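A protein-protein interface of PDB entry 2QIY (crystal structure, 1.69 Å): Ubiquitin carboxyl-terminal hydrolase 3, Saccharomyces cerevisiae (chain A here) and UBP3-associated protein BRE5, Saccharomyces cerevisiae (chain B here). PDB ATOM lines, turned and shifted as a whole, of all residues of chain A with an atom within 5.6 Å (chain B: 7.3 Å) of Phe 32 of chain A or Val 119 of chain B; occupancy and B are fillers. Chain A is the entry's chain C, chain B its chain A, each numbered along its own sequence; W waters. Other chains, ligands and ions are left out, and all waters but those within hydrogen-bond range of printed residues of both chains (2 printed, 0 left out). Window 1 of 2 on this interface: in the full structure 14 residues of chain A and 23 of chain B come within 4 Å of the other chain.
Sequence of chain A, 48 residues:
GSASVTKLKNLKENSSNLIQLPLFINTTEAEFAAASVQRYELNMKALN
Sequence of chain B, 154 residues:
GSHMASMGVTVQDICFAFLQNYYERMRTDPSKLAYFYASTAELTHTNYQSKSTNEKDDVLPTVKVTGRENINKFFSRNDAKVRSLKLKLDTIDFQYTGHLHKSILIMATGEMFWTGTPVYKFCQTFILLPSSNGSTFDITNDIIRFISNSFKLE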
ATOM      1  N   PHE A  24     -36.384 -18.302 -10.632  1.00  0.00           N
ATOM      2  CA  PHE A  24     -35.240 -19.212 -10.541  1.00  0.00           C
ATOM      3  C   PHE A  24     -35.620 -20.331  -9.595  1.00  0.00           C
ATOM      4  O   PHE A  24     -36.095 -20.075  -8.468  1.00  0.00           O
ATOM      5  CB  PHE A  24     -33.991 -18.440 -10.089  1.00  0.00           C
ATOM      6  CG  PHE A  24     -33.603 -17.389 -11.071  1.00  0.00           C
ATOM      7  CD1 PHE A  24     -34.135 -16.103 -10.986  1.00  0.00           C
ATOM      8  CD2 PHE A  24     -32.809 -17.727 -12.162  1.00  0.00           C
ATOM      9  CE1 PHE A  24     -33.838 -15.153 -11.950  1.00  0.00           C
ATOM     10  CE2 PHE A  24     -32.500 -16.782 -13.132  1.00  0.00           C
ATOM     11  CZ  PHE A  24     -33.002 -15.497 -13.018  1.00  0.00           C
ATOM     12  N   THR A  27     -32.051 -22.798  -7.839  1.00  0.00           N
ATOM     13  CA  THR A  27     -30.869 -22.044  -8.194  1.00  0.00           C
ATOM     14  C   THR A  27     -31.077 -20.566  -7.904  1.00  0.00           C
ATOM     15  O   THR A  27     -32.124 -20.146  -7.398  1.00  0.00           O
ATOM     16  CB  THR A  27     -30.491 -22.258  -9.704  1.00  0.00           C
ATOM     17  OG1 THR A  27     -29.200 -21.680  -9.968  1.00  0.00           O
ATOM     18  CG2 THR A  27     -31.523 -21.609 -10.618  1.00  0.00           C
ATOM     19  N   THR A  28     -30.041 -19.796  -8.190  1.00  0.00           N
ATOM     20  CA  THR A  28     -30.042 -18.374  -7.976  1.00  0.00           C
ATOM     21  C   THR A  28     -29.782 -17.725  -9.322  1.00  0.00           C
ATOM     22  O   THR A  28     -29.319 -18.381 -10.275  1.00  0.00           O
ATOM     23  CB  THR A  28     -28.917 -17.978  -7.026  1.00  0.00           C
ATOM     24  OG1 THR A  28     -27.654 -18.365  -7.589  1.00  0.00           O
ATOM     25  CG2 THR A  28     -29.081 -18.651  -5.655  1.00  0.00           C
ATOM     26  N   GLU A  29     -30.046 -16.426  -9.397  1.00  0.00           N
ATOM     27  CA  GLU A  29     -29.767 -15.678 -10.605  1.00  0.00           C
ATOM     28  C   GLU A  29     -28.282 -15.752 -10.975  1.00  0.00           C
ATOM     29  O   GLU A  29     -27.945 -15.878 -12.158  1.00  0.00           O
ATOM     30  CB  GLU A  29     -30.204 -14.221 -10.437  1.00  0.00           C
ATOM     31  CG  GLU A  29     -30.086 -13.454 -11.731  1.00  0.00           C
ATOM     32  CD  GLU A  29     -30.889 -12.175 -11.748  1.00  0.00           C
ATOM     33  OE1 GLU A  29     -31.465 -11.789 -10.700  1.00  0.00           O
ATOM     34  OE2 GLU A  29     -30.945 -11.557 -12.837  1.00  0.00           O
ATOM     35  N   ALA A  30     -27.406 -15.733  -9.970  1.00  0.00           N
ATOM     36  CA  ALA A  30     -25.951 -15.761 -10.218  1.00  0.00           C
ATOM     37  C   ALA A  30     -25.454 -17.085 -10.813  1.00  0.00           C
ATOM     38  O   ALA A  30     -24.611 -17.103 -11.734  1.00  0.00           O
ATOM     39  CB  ALA A  30     -25.181 -15.441  -8.933  1.00  0.00           C
ATOM     40  N   GLU A  31     -25.965 -18.186 -10.268  1.00  0.00           N
ATOM     41  CA  GLU A  31     -25.644 -19.527 -10.781  1.00  0.00           C
ATOM     42  C   GLU A  31     -26.156 -19.658 -12.211  1.00  0.00           C
ATOM     43  O   GLU A  31     -25.454 -20.169 -13.103  1.00  0.00           O
ATOM     44  CB  GLU A  31     -26.310 -20.611  -9.932  1.00  0.00           C
ATOM     45  CG  GLU A  31     -25.726 -20.831  -8.574  1.00  0.00           C
ATOM     46  CD  GLU A  31     -26.148 -22.177  -8.000  1.00  0.00           C
ATOM     47  OE1 GLU A  31     -25.581 -22.565  -6.964  1.00  0.00           O
ATOM     48  OE2 GLU A  31     -27.020 -22.847  -8.584  1.00  0.00           O
ATOM     49  N   PHE A  32     -27.391 -19.202 -12.430  1.00  0.00           N
ATOM     50  CA  PHE A  32     -27.952 -19.188 -13.774  1.00  0.00           C
ATOM     51  C   PHE A  32     -27.075 -18.380 -14.746  1.00  0.00           C
ATOM     52  O   PHE A  32     -26.759 -18.837 -15.852  1.00  0.00           O
ATOM     53  CB  PHE A  32     -29.386 -18.641 -13.821  1.00  0.00           C
ATOM     54  CG  PHE A  32     -29.834 -18.388 -15.226  1.00  0.00           C
ATOM     55  CD1 PHE A  32     -30.226 -19.458 -16.027  1.00  0.00           C
ATOM     56  CD2 PHE A  32     -29.768 -17.103 -15.780  1.00  0.00           C
ATOM     57  CE1 PHE A  32     -30.589 -19.240 -17.361  1.00  0.00           C
ATOM     58  CE2 PHE A  32     -30.138 -16.892 -17.142  1.00  0.00           C
ATOM     59  CZ  PHE A  32     -30.535 -17.960 -17.898  1.00  0.00           C
ATOM     60  N   ALA A  33     -26.671 -17.189 -14.315  1.00  0.00           N
ATOM     61  CA  ALA A  33     -25.828 -16.319 -15.143  1.00  0.00           C
ATOM     62  C   ALA A  33     -24.538 -17.014 -15.557  1.00  0.00           C
ATOM     63  O   ALA A  33     -24.095 -16.872 -16.698  1.00  0.00           O
ATOM     64  CB  ALA A  33     -25.534 -15.028 -14.400  1.00  0.00           C
ATOM     65  N   ALA A  34     -23.949 -17.771 -14.632  1.00  0.00           N
ATOM     66  CA  ALA A  34     -22.730 -18.535 -14.930  1.00  0.00           C
ATOM     67  C   ALA A  34     -22.950 -19.604 -16.002  1.00  0.00           C
ATOM     68  O   ALA A  34     -22.106 -19.809 -16.905  1.00  0.00           O
ATOM     69  CB  ALA A  34     -22.172 -19.167 -13.655  1.00  0.00           C
ATOM     70  N   ALA A  35     -24.065 -20.325 -15.877  1.00  0.00           N
ATOM     71  CA  ALA A  35     -24.423 -21.372 -16.846  1.00  0.00           C
ATOM     72  C   ALA A  35     -24.702 -20.753 -18.205  1.00  0.00           C
ATOM     73  O   ALA A  35     -24.374 -21.327 -19.254  1.00  0.00           O
ATOM     74  CB  ALA A  35     -25.645 -22.135 -16.369  1.00  0.00           C
ATOM     75  N   SER A  36     -25.302 -19.566 -18.182  1.00  0.00           N
ATOM     76  CA  SER A  36     -25.601 -18.875 -19.416  1.00  0.00           C
ATOM     77  C   SER A  36     -24.328 -18.480 -20.168  1.00  0.00           C
ATOM     78  O   SER A  36     -24.233 -18.747 -21.365  1.00  0.00           O
ATOM     79  CB  SER A  36     -26.487 -17.654 -19.149  1.00  0.00           C
ATOM     80  OG  SER A  36     -26.806 -16.990 -20.365  1.00  0.00           O
ATOM     81  N   VAL A  37     -23.376 -17.839 -19.486  1.00  0.00           N
ATOM     82  CA  VAL A  37     -22.115 -17.503 -20.146  1.00  0.00           C
ATOM     83  C   VAL A  37     -21.328 -18.736 -20.584  1.00  0.00           C
ATOM     84  O   VAL A  37     -20.701 -18.703 -21.642  1.00  0.00           O
ATOM     85  CB  VAL A  37     -21.259 -16.527 -19.328  1.00  0.00           C
ATOM     86  CG1 VAL A  37     -20.656 -17.233 -18.165  1.00  0.00           C
ATOM     87  CG2 VAL A  37     -20.186 -15.910 -20.252  1.00  0.00           C
ATOM     88  N   ARG A  39     -22.629 -21.354 -21.827  1.00  0.00           N
ATOM     89  CA  ARG A  39     -23.239 -21.674 -23.117  1.00  0.00           C
ATOM     90  C   ARG A  39     -22.657 -20.775 -24.203  1.00  0.00           C
ATOM     91  O   ARG A  39     -22.280 -21.237 -25.282  1.00  0.00           O
ATOM     92  CB  ARG A  39     -24.752 -21.500 -23.063  1.00  0.00           C
ATOM     93  CG  ARG A  39     -25.442 -21.575 -24.439  1.00  0.00           C
ATOM     94  CD  ARG A  39     -25.116 -22.881 -25.180  1.00  0.00           C
ATOM     95  NE  ARG A  39     -25.643 -24.035 -24.461  1.00  0.00           N
ATOM     96  CZ  ARG A  39     -25.162 -25.267 -24.539  1.00  0.00           C
ATOM     97  NH1 ARG A  39     -24.109 -25.528 -25.310  1.00  0.00           N
ATOM     98  NH2 ARG A  39     -25.727 -26.240 -23.833  1.00  0.00           N
ATOM     99  N   LYS B  56     -20.469 -26.973 -28.532  1.00  0.00           N
ATOM    100  CA  LYS B  56     -21.098 -28.260 -28.396  1.00  0.00           C
ATOM    101  C   LYS B  56     -22.625 -28.088 -28.474  1.00  0.00           C
ATOM    102  O   LYS B  56     -23.151 -26.988 -28.735  1.00  0.00           O
ATOM    103  CB  LYS B  56     -20.664 -28.969 -27.099  1.00  0.00           C
ATOM    104  CG  LYS B  56     -21.201 -28.334 -25.823  1.00  0.00           C
ATOM    105  CD  LYS B  56     -21.384 -29.358 -24.716  1.00  0.00           C
ATOM    106  CE  LYS B  56     -22.156 -28.752 -23.540  1.00  0.00           C
ATOM    107  NZ  LYS B  56     -21.623 -29.211 -22.206  1.00  0.00           N
ATOM    108  N   ASP B  57     -23.322 -29.193 -28.256  1.00  0.00           N
ATOM    109  CA  ASP B  57     -24.759 -29.274 -28.467  1.00  0.00           C
ATOM    110  C   ASP B  57     -25.512 -28.363 -27.529  1.00  0.00           C
ATOM    111  O   ASP B  57     -25.281 -28.379 -26.328  1.00  0.00           O
ATOM    112  CB  ASP B  57     -25.254 -30.701 -28.216  1.00  0.00           C
ATOM    113  CG  ASP B  57     -24.594 -31.738 -29.120  1.00  0.00           C
ATOM    114  OD1 ASP B  57     -24.749 -32.951 -28.817  1.00  0.00           O
ATOM    115  OD2 ASP B  57     -23.946 -31.360 -30.126  1.00  0.00           O
ATOM    116  N   ASP B  58     -26.436 -27.582 -28.070  1.00  0.00           N
ATOM    117  CA  ASP B  58     -27.258 -26.785 -27.188  1.00  0.00           C
ATOM    118  C   ASP B  58     -28.662 -27.357 -27.092  1.00  0.00           C
ATOM    119  O   ASP B  58     -29.572 -26.712 -26.585  1.00  0.00           O
ATOM    120  CB  ASP B  58     -27.225 -25.311 -27.579  1.00  0.00           C
ATOM    121  CG  ASP B  58     -28.001 -25.007 -28.854  1.00  0.00           C
ATOM    122  OD1 ASP B  58     -28.270 -23.806 -29.060  1.00  0.00           O
ATOM    123  OD2 ASP B  58     -28.356 -25.946 -29.614  1.00  0.00           O
ATOM    124  N   VAL B  59     -28.825 -28.594 -27.570  1.00  0.00           N
ATOM    125  CA  VAL B  59     -30.021 -29.364 -27.247  1.00  0.00           C
ATOM    126  C   VAL B  59     -29.637 -30.731 -26.672  1.00  0.00           C
ATOM    127  O   VAL B  59     -28.495 -31.192 -26.820  1.00  0.00           O
ATOM    128  CB  VAL B  59     -30.959 -29.568 -28.463  1.00  0.00           C
ATOM    129  CG1 VAL B  59     -31.464 -28.227 -29.006  1.00  0.00           C
ATOM    130  CG2 VAL B  59     -30.263 -30.406 -29.566  1.00  0.00           C
ATOM    131  N   LYS B  86     -31.673 -27.485 -12.438  1.00  0.00           N
ATOM    132  CA  LYS B  86     -31.896 -26.093 -12.079  1.00  0.00           C
ATOM    133  C   LYS B  86     -32.558 -25.418 -13.286  1.00  0.00           C
ATOM    134  O   LYS B  86     -32.418 -25.859 -14.426  1.00  0.00           O
ATOM    135  CB  LYS B  86     -30.542 -25.445 -11.787  1.00  0.00           C
ATOM    136  CG  LYS B  86     -29.849 -26.038 -10.538  1.00  0.00           C
ATOM    137  CD  LYS B  86     -28.404 -25.596 -10.413  1.00  0.00           C
ATOM    138  CE  LYS B  86     -27.769 -26.243  -9.206  1.00  0.00           C
ATOM    139  NZ  LYS B  86     -28.011 -25.410  -8.009  1.00  0.00           N
ATOM    140  N   LEU B  87     -33.305 -24.351 -13.051  1.00  0.00           N
ATOM    141  CA  LEU B  87     -33.876 -23.649 -14.206  1.00  0.00           C
ATOM    142  C   LEU B  87     -34.254 -22.230 -13.914  1.00  0.00           C
ATOM    143  O   LEU B  87     -34.469 -21.858 -12.754  1.00  0.00           O
ATOM    144  CB  LEU B  87     -35.092 -24.378 -14.814  1.00  0.00           C
ATOM    145  CG  LEU B  87     -36.383 -24.427 -13.988  1.00  0.00           C
ATOM    146  CD1 LEU B  87     -37.575 -24.609 -14.944  1.00  0.00           C
ATOM    147  CD2 LEU B  87     -36.298 -25.564 -12.960  1.00  0.00           C
ATOM    148  N   LYS B  88     -34.307 -21.469 -15.002  1.00  0.00           N
ATOM    149  CA  LYS B  88     -34.973 -20.177 -15.049  1.00  0.00           C
ATOM    150  C   LYS B  88     -36.294 -20.415 -15.764  1.00  0.00           C
ATOM    151  O   LYS B  88     -36.312 -20.831 -16.930  1.00  0.00           O
ATOM    152  CB  LYS B  88     -34.115 -19.174 -15.808  1.00  0.00           C
ATOM    153  CG  LYS B  88     -34.787 -17.829 -15.986  1.00  0.00           C
ATOM    154  CD  LYS B  88     -33.864 -16.814 -16.650  1.00  0.00           C
ATOM    155  CE  LYS B  88     -34.586 -15.486 -16.791  1.00  0.00           C
ATOM    156  NZ  LYS B  88     -33.686 -14.428 -17.328  1.00  0.00           N
ATOM    157  N   LEU B  89     -37.398 -20.255 -15.040  1.00  0.00           N
ATOM    158  CA  LEU B  89     -38.746 -20.451 -15.626  1.00  0.00           C
ATOM    159  C   LEU B  89     -39.185 -19.097 -16.193  1.00  0.00           C
ATOM    160  O   LEU B  89     -39.331 -18.131 -15.439  1.00  0.00           O
ATOM    161  CB  LEU B  89     -39.735 -20.908 -14.535  1.00  0.00           C
ATOM    162  CG  LEU B  89     -40.995 -21.753 -14.780  1.00  0.00           C
ATOM    163  CD1 LEU B  89     -42.171 -21.289 -13.932  1.00  0.00           C
ATOM    164  CD2 LEU B  89     -41.366 -22.098 -16.256  1.00  0.00           C
ATOM    165  N   ASP B  90     -39.375 -19.016 -17.515  1.00  0.00           N
ATOM    166  CA  ASP B  90     -39.680 -17.734 -18.179  1.00  0.00           C
ATOM    167  C   ASP B  90     -41.183 -17.468 -18.376  1.00  0.00           C
ATOM    168  O   ASP B  90     -41.653 -16.336 -18.210  1.00  0.00           O
ATOM    169  CB  ASP B  90     -39.041 -17.669 -19.567  1.00  0.00           C
ATOM    170  CG  ASP B  90     -37.522 -17.497 -19.535  1.00  0.00           C
ATOM    171  OD1 ASP B  90     -36.887 -18.083 -20.424  1.00  0.00           O
ATOM    172  OD2 ASP B  90     -36.970 -16.768 -18.679  1.00  0.00           O
ATOM    173  N   GLY B 110     -38.342 -21.996 -20.669  1.00  0.00           N
ATOM    174  CA  GLY B 110     -37.288 -21.392 -19.851  1.00  0.00           C
ATOM    175  C   GLY B 110     -35.934 -21.877 -20.296  1.00  0.00           C
ATOM    176  O   GLY B 110     -35.775 -22.336 -21.435  1.00  0.00           O
ATOM    177  N   GLU B 111     -34.977 -21.795 -19.381  1.00  0.00           N
ATOM    178  CA  GLU B 111     -33.610 -22.245 -19.634  1.00  0.00           C
ATOM    179  C   GLU B 111     -33.209 -23.149 -18.479  1.00  0.00           C
ATOM    180  O   GLU B 111     -33.322 -22.771 -17.322  1.00  0.00           O
ATOM    181  CB  GLU B 111     -32.673 -21.053 -19.818  1.00  0.00           C
ATOM    182  CG  GLU B 111     -33.053 -20.252 -21.083  1.00  0.00           C
ATOM    183  CD  GLU B 111     -32.020 -19.241 -21.562  1.00  0.00           C
ATOM    184  OE1 GLU B 111     -30.912 -19.140 -20.996  1.00  0.00           O
ATOM    185  OE2 GLU B 111     -32.336 -18.595 -22.599  1.00  0.00           O
ATOM    186  N   MET B 112     -32.832 -24.374 -18.831  1.00  0.00           N
ATOM    187  CA  MET B 112     -32.578 -25.431 -17.867  1.00  0.00           C
ATOM    188  C   MET B 112     -31.090 -25.741 -17.842  1.00  0.00           C
ATOM    189  O   MET B 112     -30.412 -25.673 -18.865  1.00  0.00           O
ATOM    190  CB  MET B 112     -33.393 -26.682 -18.286  1.00  0.00           C
ATOM    191  CG  MET B 112     -33.282 -27.833 -17.339  1.00  0.00           C
ATOM    192  SD  MET B 112     -34.465 -29.099 -17.841  1.00  0.00           S
ATOM    193  CE  MET B 112     -35.996 -28.325 -17.353  1.00  0.00           C
ATOM    194  N   PHE B 113     -30.565 -26.067 -16.672  1.00  0.00           N
ATOM    195  CA  PHE B 113     -29.182 -26.536 -16.597  1.00  0.00           C
ATOM    196  C   PHE B 113     -29.063 -27.470 -15.400  1.00  0.00           C
ATOM    197  O   PHE B 113     -30.050 -27.717 -14.687  1.00  0.00           O
ATOM    198  CB  PHE B 113     -28.171 -25.387 -16.550  1.00  0.00           C
ATOM    199  CG  PHE B 113     -28.269 -24.502 -15.315  1.00  0.00           C
ATOM    200  CD1 PHE B 113     -27.265 -24.557 -14.342  1.00  0.00           C
ATOM    201  CD2 PHE B 113     -29.312 -23.594 -15.168  1.00  0.00           C
ATOM    202  CE1 PHE B 113     -27.328 -23.751 -13.219  1.00  0.00           C
ATOM    203  CE2 PHE B 113     -29.374 -22.741 -14.020  1.00  0.00           C
ATOM    204  CZ  PHE B 113     -28.385 -22.840 -13.065  1.00  0.00           C
ATOM    205  N   TRP B 114     -27.886 -28.056 -15.251  1.00  0.00           N
ATOM    206  CA  TRP B 114     -27.601 -28.888 -14.090  1.00  0.00           C
ATOM    207  C   TRP B 114     -26.338 -28.312 -13.484  1.00  0.00           C
ATOM    208  O   TRP B 114     -25.585 -27.571 -14.146  1.00  0.00           O
ATOM    209  CB  TRP B 114     -27.433 -30.354 -14.523  1.00  0.00           C
ATOM    210  CG  TRP B 114     -28.737 -30.965 -15.045  1.00  0.00           C
ATOM    211  CD1 TRP B 114     -29.583 -31.820 -14.364  1.00  0.00           C
ATOM    212  CD2 TRP B 114     -29.328 -30.755 -16.322  1.00  0.00           C
ATOM    213  NE1 TRP B 114     -30.664 -32.136 -15.145  1.00  0.00           N
ATOM    214  CE2 TRP B 114     -30.538 -31.499 -16.355  1.00  0.00           C
ATOM    215  CE3 TRP B 114     -28.953 -30.014 -17.463  1.00  0.00           C
ATOM    216  CZ2 TRP B 114     -31.373 -31.530 -17.487  1.00  0.00           C
ATOM    217  CZ3 TRP B 114     -29.810 -30.030 -18.590  1.00  0.00           C
ATOM    218  CH2 TRP B 114     -30.999 -30.775 -18.578  1.00  0.00           C
ATOM    219  N   THR B 117     -23.222 -27.179 -15.606  1.00  0.00           N
ATOM    220  CA  THR B 117     -23.401 -27.294 -17.059  1.00  0.00           C
ATOM    221  C   THR B 117     -23.828 -25.968 -17.673  1.00  0.00           C
ATOM    222  O   THR B 117     -24.291 -25.078 -16.953  1.00  0.00           O
ATOM    223  CB  THR B 117     -24.456 -28.349 -17.481  1.00  0.00           C
ATOM    224  OG1 THR B 117     -25.779 -27.813 -17.358  1.00  0.00           O
ATOM    225  CG2 THR B 117     -24.310 -29.638 -16.679  1.00  0.00           C
ATOM    226  N   PRO B 118     -23.689 -25.829 -19.012  1.00  0.00           N
ATOM    227  CA  PRO B 118     -24.318 -24.669 -19.653  1.00  0.00           C
ATOM    228  C   PRO B 118     -25.836 -24.802 -19.652  1.00  0.00           C
ATOM    229  O   PRO B 118     -26.377 -25.878 -19.357  1.00  0.00           O
ATOM    230  CB  PRO B 118     -23.813 -24.721 -21.096  1.00  0.00           C
ATOM    231  CG  PRO B 118     -23.373 -26.123 -21.292  1.00  0.00           C
ATOM    232  CD  PRO B 118     -22.956 -26.674 -19.978  1.00  0.00           C
ATOM    233  N   VAL B 119     -26.518 -23.719 -20.023  1.00  0.00           N
ATOM    234  CA  VAL B 119     -27.979 -23.761 -20.146  1.00  0.00           C
ATOM    235  C   VAL B 119     -28.427 -24.398 -21.479  1.00  0.00           C
ATOM    236  O   VAL B 119     -27.670 -24.453 -22.466  1.00  0.00           O
ATOM    237  CB  VAL B 119     -28.613 -22.372 -20.084  1.00  0.00           C
ATOM    238  CG1 VAL B 119     -28.356 -21.745 -18.707  1.00  0.00           C
ATOM    239  CG2 VAL B 119     -28.057 -21.469 -21.226  1.00  0.00           C
ATOM    240  N   TYR B 120     -29.686 -24.847 -21.460  1.00  0.00           N
ATOM    241  CA  TYR B 120     -30.385 -25.367 -22.618  1.00  0.00           C
ATOM    242  C   TYR B 120     -31.794 -24.789 -22.580  1.00  0.00           C
ATOM    243  O   TYR B 120     -32.473 -24.865 -21.532  1.00  0.00           O
ATOM    244  CB  TYR B 120     -30.511 -26.877 -22.501  1.00  0.00           C
ATOM    245  CG  TYR B 120     -29.197 -27.603 -22.441  1.00  0.00           C
ATOM    246  CD1 TYR B 120     -28.501 -27.727 -21.246  1.00  0.00           C
ATOM    247  CD2 TYR B 120     -28.652 -28.163 -23.595  1.00  0.00           C
ATOM    248  CE1 TYR B 120     -27.289 -28.416 -21.171  1.00  0.00           C
ATOM    249  CE2 TYR B 120     -27.457 -28.853 -23.555  1.00  0.00           C
ATOM    250  CZ  TYR B 120     -26.761 -28.972 -22.328  1.00  0.00           C
ATOM    251  OH  TYR B 120     -25.546 -29.626 -22.271  1.00  0.00           O
ATOM    252  N   LYS B 121     -32.241 -24.220 -23.691  1.00  0.00           N
ATOM    253  CA  LYS B 121     -33.588 -23.636 -23.770  1.00  0.00           C
ATOM    254  C   LYS B 121     -34.553 -24.783 -23.853  1.00  0.00           C
ATOM    255  O   LYS B 121     -34.246 -25.778 -24.513  1.00  0.00           O
ATOM    256  CB  LYS B 121     -33.751 -22.844 -25.048  1.00  0.00           C
ATOM    257  CG  LYS B 121     -33.169 -21.448 -24.998  1.00  0.00           C
ATOM    258  CD  LYS B 121     -33.930 -20.621 -26.055  1.00  0.00           C
ATOM    259  CE  LYS B 121     -33.956 -19.126 -25.724  1.00  0.00           C
ATOM    260  NZ  LYS B 121     -34.526 -18.769 -24.409  1.00  0.00           N
ATOM    261  N   PHE B 146     -36.049 -29.682 -26.002  1.00  0.00           N
ATOM    262  CA  PHE B 146     -34.990 -28.674 -26.023  1.00  0.00           C
ATOM    263  C   PHE B 146     -34.925 -27.980 -27.369  1.00  0.00           C
ATOM    264  O   PHE B 146     -35.101 -28.599 -28.418  1.00  0.00           O
ATOM    265  CB  PHE B 146     -33.648 -29.303 -25.599  1.00  0.00           C
ATOM    266  CG  PHE B 146     -33.691 -29.807 -24.204  1.00  0.00           C
ATOM    267  CD1 PHE B 146     -33.501 -28.923 -23.128  1.00  0.00           C
ATOM    268  CD2 PHE B 146     -33.983 -31.141 -23.931  1.00  0.00           C
ATOM    269  CE1 PHE B 146     -33.589 -29.390 -21.817  1.00  0.00           C
ATOM    270  CE2 PHE B 146     -34.077 -31.623 -22.618  1.00  0.00           C
ATOM    271  CZ  PHE B 146     -33.873 -30.738 -21.544  1.00  0.00           C
HETATM  272  O   HOH W   1     -22.863 -24.639 -27.399  1.00  0.00           O
HETATM  273  O   HOH W   2     -29.223 -17.160 -21.230  1.00  0.00           O
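OE2 of Glu 31 of chain A lies within salt-bridge range of NZ of Lys 86 of chain B, 2.8 Å away.
N of Val 119 of chain B lies within hydrogen-bond range of O of Ala 35 of chain A.
NH1 of Arg 39 of chain A sits at hydrogen-bond distance from O of Asp 57 of chain B, at 3.2 Å.
The backbone carbonyl oxygen (O) of Val 119 of chain B is in hydrogen-bond range of the guanidinium group (NE) of Arg 39 of chain A.
The backbone NH (N) of Lys 88 of chain B sits at hydrogen-bond distance from the backbone carbonyl oxygen (O) of Glu 111 of chain B (2.8 Å).
OG1 of Thr 27 of chain A lies within hydrogen-bond range of OE2 of Glu 31 of chain A (2.8 Å).
The backbone NH of Trp 114 of chain B is in hydrogen-bond range of the side-chain hydroxyl of Thr 117 of chain B, at 3.0 Å.
The side-chain hydroxyl (OG1) of Thr 28 of chain A is in hydrogen-bond range of the backbone NH (N) of Glu 31 of chain A, 3.2 Å away.
O of Tyr 120 of chain B is in hydrogen-bond range of N of Met 112 of chain B, 2.8 Å away.
NZ of Lys 121 of chain B is in salt-bridge range of OE2 of Glu 111 of chain B.
Among the printed residues, pairs that only touch across the chains: Phe 24 of chain A with Leu 87 of chain B (3.5 Å), Phe 24 of chain A with Lys 88 of chain B (3.8 Å), Thr 27 of chain A with Lys 86 of chain B (3.8 Å), Thr 27 of chain A with Leu 87 of chain B (3.6 Å), Thr 27 of chain A with Phe 113 of chain B (3.4 Å), Glu 31 of chain A with Phe 113 of chain B (3.97 Å), Phe 32 of chain A with Lys 88 of chain B (3.7 Å), Phe 32 of chain A with Glu 111 of chain B (3.3 Å), Phe 32 of chain A with Phe 113 of chain B (3.7 Å), Phe 32 of chain A with Val 119 of chain B (3.6 Å), Ala 35 of chain A with Phe 113 of chain B (3.5 Å), Ala 35 of chain A with Thr 117 of chain B (3.3 Å), Ala 35 of chain A with Pro 118 of chain B (3.4 Å), Ser 36 of chain A with Val 119 of chain B (3.8 Å), Arg 39 of chain A with Lys 56 of chain B (3.8 Å), Arg 39 of chain A with Asp 58 of chain B (3.7 Å), Arg 39 of chain A with Pro 118 of chain B (3.5 Å) and Arg 39 of chain A with Tyr 120 of chain B (3.1 Å).
Of the printed residues of chain B, Phe 24 of chain A touches Leu 87 and Lys 88.
Of the printed residues of chain A, Asp 57 of chain B touches Arg 39 (3.2 Å).
Of the printed residues of chain A, Lys 86 of chain B touches Thr 27 and Glu 31.
Printed residues of chain A within 4 Å of Pro 118 of chain B: Ala 35 and Arg 39.
Val 119 of chain B touches just these residues of chain A: Phe 32, Ala 35, Ser 36 and Arg 39.
Lys 121 of chain B touches none of the printed residues of chain A.
The nearest residue of chain B that does not touch Phe 32 of chain A is Leu 87 of chain B (5.3 Å).
The nearest printed residue of chain A that does not touch Lys 56 of chain B is Ala 35 of chain A (8.9 Å).
Of the 20 printed residues of chain B, 12 touch a printed residue of chain A.
Hydrophobic or aromatic side chains of chain B within 4 Å of the printed part of chain A: Phe 113, Pro 118, Val 119 and Tyr 120.
Of the 13 printed residues of chain A, 7 touch a printed residue of chain B.
Among the printed residues, 22 pairs touch across the chains.
Among the printed residues, Asp or Glu carboxylates within 4 Å of a Lys or Arg side-chain nitrogen of the other chain: Glu 31 of chain A with Lys 86 of chain B.
Water W2 lies within hydrogen-bond range of the side-chain hydroxyl of Ser 36 of chain A (2.6 Å) and the side-chain carboxylate of Glu 111 of chain B (2.6 Å).
Water W1 bridges NH1 of Arg 39 of chain A (2.6 Å) and O of Lys 56 of chain B (2.7 Å).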
